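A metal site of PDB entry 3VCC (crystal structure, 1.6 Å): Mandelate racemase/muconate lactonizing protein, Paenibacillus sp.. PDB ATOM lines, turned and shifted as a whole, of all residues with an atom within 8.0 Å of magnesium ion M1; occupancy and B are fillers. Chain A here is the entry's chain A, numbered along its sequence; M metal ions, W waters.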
ATOM      1  N   ASN A 209     -12.092  14.169 -10.300  1.00  0.00           N
ATOM      2  CA  ASN A 209     -12.368  15.362  -9.518  1.00  0.00           C
ATOM      3  C   ASN A 209     -11.728  16.605 -10.127  1.00  0.00           C
ATOM      4  O   ASN A 209     -11.149  17.433  -9.432  1.00  0.00           O
ATOM      5  CB  ASN A 209     -11.975  15.205  -8.054  1.00  0.00           C
ATOM      6  CG  ASN A 209     -12.913  14.281  -7.313  1.00  0.00           C
ATOM      7  OD1 ASN A 209     -12.612  13.106  -7.157  1.00  0.00           O
ATOM      8  ND2 ASN A 209     -14.077  14.796  -6.895  1.00  0.00           N
ATOM      9  N   ASN A 210     -11.904  16.721 -11.442  1.00  0.00           N
ATOM     10  CA  ASN A 210     -11.478  17.894 -12.228  1.00  0.00           C
ATOM     11  C   ASN A 210      -9.969  18.141 -12.307  1.00  0.00           C
ATOM     12  O   ASN A 210      -9.533  19.212 -12.760  1.00  0.00           O
ATOM     13  CB  ASN A 210     -12.215  19.156 -11.755  1.00  0.00           C
ATOM     14  CG  ASN A 210     -13.705  19.114 -12.084  1.00  0.00           C
ATOM     15  OD1 ASN A 210     -14.131  18.456 -13.044  1.00  0.00           O
ATOM     16  ND2 ASN A 210     -14.497  19.817 -11.267  1.00  0.00           N
ATOM     17  N   GLU A 233     -15.695  10.406 -15.141  1.00  0.00           N
ATOM     18  CA  GLU A 233     -16.424  11.370 -14.341  1.00  0.00           C
ATOM     19  C   GLU A 233     -15.519  12.554 -13.992  1.00  0.00           C
ATOM     20  O   GLU A 233     -14.397  12.375 -13.514  1.00  0.00           O
ATOM     21  CB  GLU A 233     -16.917  10.697 -13.053  1.00  0.00           C
ATOM     22  CG  GLU A 233     -17.471  11.664 -12.009  1.00  0.00           C
ATOM     23  CD  GLU A 233     -18.154  10.920 -10.855  1.00  0.00           C
ATOM     24  OE1 GLU A 233     -18.468   9.726 -10.994  1.00  0.00           O
ATOM     25  OE2 GLU A 233     -18.375  11.546  -9.804  1.00  0.00           O
ATOM     26  N   GLU A 234     -16.026  13.764 -14.248  1.00  0.00           N
ATOM     27  CA  GLU A 234     -15.328  14.994 -13.897  1.00  0.00           C
ATOM     28  C   GLU A 234     -13.834  14.995 -14.265  1.00  0.00           C
ATOM     29  O   GLU A 234     -12.968  15.213 -13.410  1.00  0.00           O
ATOM     30  CB  GLU A 234     -15.510  15.330 -12.410  1.00  0.00           C
ATOM     31  CG  GLU A 234     -16.976  15.636 -12.029  1.00  0.00           C
ATOM     32  CD  GLU A 234     -17.106  16.657 -10.906  1.00  0.00           C
ATOM     33  OE1 GLU A 234     -16.651  16.404  -9.776  1.00  0.00           O
ATOM     34  OE2 GLU A 234     -17.702  17.722 -11.152  1.00  0.00           O
ATOM     35  N   ALA A 235     -13.544  14.719 -15.540  1.00  0.00           N
ATOM     36  CA  ALA A 235     -12.170  14.799 -16.036  1.00  0.00           C
ATOM     37  C   ALA A 235     -11.631  16.209 -15.795  1.00  0.00           C
ATOM     38  O   ALA A 235     -10.475  16.373 -15.390  1.00  0.00           O
ATOM     39  CB  ALA A 235     -12.139  14.456 -17.538  1.00  0.00           C
ATOM     40  N   PHE A 236     -12.492  17.202 -16.031  1.00  0.00           N
ATOM     41  CA  PHE A 236     -12.184  18.625 -15.843  1.00  0.00           C
ATOM     42  C   PHE A 236     -13.541  19.319 -15.722  1.00  0.00           C
ATOM     43  O   PHE A 236     -14.565  18.738 -16.074  1.00  0.00           O
ATOM     44  CB  PHE A 236     -11.441  19.178 -17.061  1.00  0.00           C
ATOM     45  CG  PHE A 236     -11.952  18.649 -18.364  1.00  0.00           C
ATOM     46  CD1 PHE A 236     -11.295  17.598 -19.014  1.00  0.00           C
ATOM     47  CD2 PHE A 236     -13.137  19.135 -18.914  1.00  0.00           C
ATOM     48  CE1 PHE A 236     -11.783  17.090 -20.226  1.00  0.00           C
ATOM     49  CE2 PHE A 236     -13.639  18.614 -20.114  1.00  0.00           C
ATOM     50  CZ  PHE A 236     -12.951  17.591 -20.767  1.00  0.00           C
ATOM     51  N   HIS A 237     -13.570  20.553 -15.243  1.00  0.00           N
ATOM     52  CA  HIS A 237     -14.854  21.241 -15.101  1.00  0.00           C
ATOM     53  C   HIS A 237     -15.597  21.233 -16.421  1.00  0.00           C
ATOM     54  O   HIS A 237     -15.012  21.562 -17.486  1.00  0.00           O
ATOM     55  CB  HIS A 237     -14.682  22.664 -14.582  1.00  0.00           C
ATOM     56  CG  HIS A 237     -15.991  23.345 -14.305  1.00  0.00           C
ATOM     57  ND1 HIS A 237     -16.892  22.882 -13.371  1.00  0.00           N
ATOM     58  CD2 HIS A 237     -16.560  24.430 -14.879  1.00  0.00           C
ATOM     59  CE1 HIS A 237     -17.951  23.669 -13.357  1.00  0.00           C
ATOM     60  NE2 HIS A 237     -17.776  24.617 -14.269  1.00  0.00           N
ATOM     61  N   GLU A 238     -16.872  20.867 -16.366  1.00  0.00           N
ATOM     62  CA  GLU A 238     -17.688  20.713 -17.583  1.00  0.00           C
ATOM     63  C   GLU A 238     -17.574  21.950 -18.471  1.00  0.00           C
ATOM     64  O   GLU A 238     -17.635  23.088 -17.995  1.00  0.00           O
ATOM     65  CB  GLU A 238     -19.151  20.454 -17.227  1.00  0.00           C
ATOM     66  CG  GLU A 238     -19.714  21.461 -16.219  1.00  0.00           C
ATOM     67  CD  GLU A 238     -19.729  20.904 -14.797  1.00  0.00           C
ATOM     68  OE1 GLU A 238     -20.707  21.117 -14.062  1.00  0.00           O
ATOM     69  OE2 GLU A 238     -18.737  20.249 -14.413  1.00  0.00           O
ATOM     70  N   ASP A 239     -17.401  21.709 -19.760  1.00  0.00           N
ATOM     71  CA  ASP A 239     -17.197  22.759 -20.747  1.00  0.00           C
ATOM     72  C   ASP A 239     -17.721  22.158 -22.048  1.00  0.00           C
ATOM     73  O   ASP A 239     -17.244  21.088 -22.464  1.00  0.00           O
ATOM     74  CB  ASP A 239     -15.699  23.075 -20.856  1.00  0.00           C
ATOM     75  CG  ASP A 239     -15.387  24.144 -21.898  1.00  0.00           C
ATOM     76  OD1 ASP A 239     -16.043  24.158 -22.963  1.00  0.00           O
ATOM     77  OD2 ASP A 239     -14.479  24.975 -21.664  1.00  0.00           O
ATOM     78  N   TYR A 243     -15.876  18.879 -24.028  1.00  0.00           N
ATOM     79  CA  TYR A 243     -16.575  17.585 -24.068  1.00  0.00           C
ATOM     80  C   TYR A 243     -16.998  17.225 -25.505  1.00  0.00           C
ATOM     81  O   TYR A 243     -16.984  16.052 -25.872  1.00  0.00           O
ATOM     82  CB  TYR A 243     -17.799  17.588 -23.140  1.00  0.00           C
ATOM     83  CG  TYR A 243     -17.494  17.231 -21.705  1.00  0.00           C
ATOM     84  CD1 TYR A 243     -16.430  16.387 -21.377  1.00  0.00           C
ATOM     85  CD2 TYR A 243     -18.288  17.722 -20.675  1.00  0.00           C
ATOM     86  CE1 TYR A 243     -16.169  16.050 -20.053  1.00  0.00           C
ATOM     87  CE2 TYR A 243     -18.036  17.388 -19.351  1.00  0.00           C
ATOM     88  CZ  TYR A 243     -16.980  16.557 -19.042  1.00  0.00           C
ATOM     89  OH  TYR A 243     -16.754  16.243 -17.735  1.00  0.00           O
ATOM     90  N   ALA A 260     -19.603  11.418 -17.556  1.00  0.00           N
ATOM     91  CA  ALA A 260     -20.458  11.629 -16.377  1.00  0.00           C
ATOM     92  C   ALA A 260     -20.052  12.925 -15.680  1.00  0.00           C
ATOM     93  O   ALA A 260     -18.878  13.193 -15.509  1.00  0.00           O
ATOM     94  CB  ALA A 260     -20.327  10.449 -15.423  1.00  0.00           C
ATOM     95  N   ASP A 261     -21.038  13.732 -15.282  1.00  0.00           N
ATOM     96  CA  ASP A 261     -20.699  14.985 -14.600  1.00  0.00           C
ATOM     97  C   ASP A 261     -21.922  15.509 -13.828  1.00  0.00           C
ATOM     98  O   ASP A 261     -23.002  14.934 -13.949  1.00  0.00           O
ATOM     99  CB  ASP A 261     -20.222  16.010 -15.622  1.00  0.00           C
ATOM    100  CG  ASP A 261     -19.132  16.914 -15.082  1.00  0.00           C
ATOM    101  OD1 ASP A 261     -19.262  17.312 -13.907  1.00  0.00           O
ATOM    102  OD2 ASP A 261     -18.171  17.231 -15.827  1.00  0.00           O
ATOM    103  N   GLY A 262     -21.737  16.559 -13.032  1.00  0.00           N
ATOM    104  CA  GLY A 262     -22.876  17.243 -12.425  1.00  0.00           C
ATOM    105  C   GLY A 262     -22.858  17.477 -10.915  1.00  0.00           C
ATOM    106  O   GLY A 262     -23.719  18.188 -10.391  1.00  0.00           O
ATOM    107  N   GLU A 263     -21.906  16.888 -10.195  1.00  0.00           N
ATOM    108  CA  GLU A 263     -21.883  17.086  -8.750  1.00  0.00           C
ATOM    109  C   GLU A 263     -21.370  18.493  -8.400  1.00  0.00           C
ATOM    110  O   GLU A 263     -20.826  19.197  -9.245  1.00  0.00           O
ATOM    111  CB  GLU A 263     -21.046  16.023  -8.044  1.00  0.00           C
ATOM    112  CG  GLU A 263     -19.567  16.235  -8.251  1.00  0.00           C
ATOM    113  CD  GLU A 263     -18.750  15.123  -7.619  1.00  0.00           C
ATOM    114  OE1 GLU A 263     -18.050  15.355  -6.617  1.00  0.00           O
ATOM    115  OE2 GLU A 263     -18.864  14.006  -8.133  1.00  0.00           O
ATOM    116  N   GLY A 264     -21.556  18.894  -7.139  1.00  0.00           N
ATOM    117  CA  GLY A 264     -20.989  20.142  -6.640  1.00  0.00           C
ATOM    118  C   GLY A 264     -21.599  21.375  -7.286  1.00  0.00           C
ATOM    119  O   GLY A 264     -22.781  21.403  -7.612  1.00  0.00           O
ATOM    120  N   LEU A 265     -20.780  22.407  -7.490  1.00  0.00           N
ATOM    121  CA  LEU A 265     -21.285  23.607  -8.143  1.00  0.00           C
ATOM    122  C   LEU A 265     -21.210  23.435  -9.671  1.00  0.00           C
ATOM    123  O   LEU A 265     -20.224  23.809 -10.312  1.00  0.00           O
ATOM    124  CB  LEU A 265     -20.495  24.841  -7.698  1.00  0.00           C
ATOM    125  CG  LEU A 265     -20.528  25.147  -6.196  1.00  0.00           C
ATOM    126  CD1 LEU A 265     -19.508  26.229  -5.838  1.00  0.00           C
ATOM    127  CD2 LEU A 265     -21.937  25.555  -5.775  1.00  0.00           C
ATOM    128  N   ALA A 266     -22.256  22.831 -10.236  1.00  0.00           N
ATOM    129  CA  ALA A 266     -22.281  22.491 -11.650  1.00  0.00           C
ATOM    130  C   ALA A 266     -22.536  23.725 -12.507  1.00  0.00           C
ATOM    131  O   ALA A 266     -23.086  24.719 -12.033  1.00  0.00           O
ATOM    132  CB  ALA A 266     -23.356  21.450 -11.921  1.00  0.00           C
ATOM    133  N   SER A 267     -22.134  23.630 -13.771  1.00  0.00           N
ATOM    134  CA  SER A 267     -22.476  24.650 -14.746  1.00  0.00           C
ATOM    135  C   SER A 267     -23.983  24.769 -14.844  1.00  0.00           C
ATOM    136  O   SER A 267     -24.682  23.747 -14.964  1.00  0.00           O
ATOM    137  CB  SER A 267     -21.933  24.302 -16.129  1.00  0.00           C
ATOM    138  OG  SER A 267     -22.492  25.201 -17.075  1.00  0.00           O
ATOM    139  N   LEU A 270     -25.278  22.730 -17.836  1.00  0.00           N
ATOM    140  CA  LEU A 270     -24.893  21.328 -18.010  1.00  0.00           C
ATOM    141  C   LEU A 270     -25.967  20.463 -18.666  1.00  0.00           C
ATOM    142  O   LEU A 270     -25.678  19.653 -19.543  1.00  0.00           O
ATOM    143  CB  LEU A 270     -24.451  20.702 -16.683  1.00  0.00           C
ATOM    144  CG  LEU A 270     -24.013  19.233 -16.668  1.00  0.00           C
ATOM    145  CD1 LEU A 270     -22.835  18.932 -17.622  1.00  0.00           C
ATOM    146  CD2 LEU A 270     -23.680  18.768 -15.231  1.00  0.00           C
ATOM    147  N   GLN A 283     -25.114  13.748 -12.451  1.00  0.00           N
ATOM    148  CA  GLN A 283     -24.728  13.306 -11.118  1.00  0.00           C
ATOM    149  C   GLN A 283     -25.020  14.284  -9.994  1.00  0.00           C
ATOM    150  O   GLN A 283     -24.304  14.336  -8.990  1.00  0.00           O
ATOM    151  CB  GLN A 283     -23.249  12.894 -11.102  1.00  0.00           C
ATOM    152  CG  GLN A 283     -22.945  11.799 -12.103  1.00  0.00           C
ATOM    153  CD  GLN A 283     -21.505  11.319 -12.020  1.00  0.00           C
ATOM    154  OE1 GLN A 283     -20.584  12.065 -12.298  1.00  0.00           O
ATOM    155  NE2 GLN A 283     -21.324  10.076 -11.603  1.00  0.00           N
HETATM  156 MG    MG M   1     -18.300  18.914 -12.842  1.00  0.00          MG
HETATM  157 MG    MG M   2     -17.316  12.521  -8.308  1.00  0.00          MG
HETATM  158  O   HOH W   1     -16.416  18.432 -13.862  1.00  0.00           O
HETATM  159  O   HOH W   2     -20.315  19.376 -11.968  1.00  0.00           O
HETATM  160  O   HOH W   3     -17.288  20.609 -11.803  1.00  0.00           O
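OE2 of Glu 238 binds magnesium ion M1 (2.1 Å). The side-chain carboxylate (OD1) of Asp 261 is bound to magnesium ion M1. Magnesium ion M1 is bound by OE2 of Glu 234 (2.2 Å). Magnesium ion M1 is bound by water W1, at 2.2 Å. Magnesium ion M1 is bound by water W3 (2.2 Å). Water W2 binds magnesium ion M1 (2.2 Å). Magnesium ion M1 has six donor atoms within binding distance.
O of Glu 234 is in hydrogen-bond range of N of Asn 209 (3.4 Å). The backbone NH (N) of Glu 234 lies within hydrogen-bond range of the backbone carbonyl oxygen (O) of Ala 260 (3.2 Å). O of Asp 261 lies within hydrogen-bond range of N of Gln 283 (2.8 Å). N of Ser 267 lies within hydrogen-bond range of OE1 of Glu 238 (2.9 Å). The backbone NH (N) of Asn 210 is in hydrogen-bond range of the backbone carbonyl oxygen (O) of Glu 234, 2.7 Å away. The side-chain carboxylate of Asp 261 sits at hydrogen-bond distance from the side-chain hydroxyl of Tyr 243 (2.6 Å). The side-chain carboxylate of Glu 238 lies close to a ring nitrogen (ND1) of His 237 (3.4 Å).
Of the 20 residues printed, 3 come within 4 Å of magnesium ion M1. The nearest printed residue that does not touch magnesium ion M1 is Gly 262 (4.2 Å).
Water W2 lies within hydrogen-bond range of OE1 of Glu 238, O of Glu 263 and N of Gly 262. Water W3 lies within hydrogen-bond range of ND1 of His 237 (2.8 Å) and ND2 of Asn 210 (3.0 Å).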
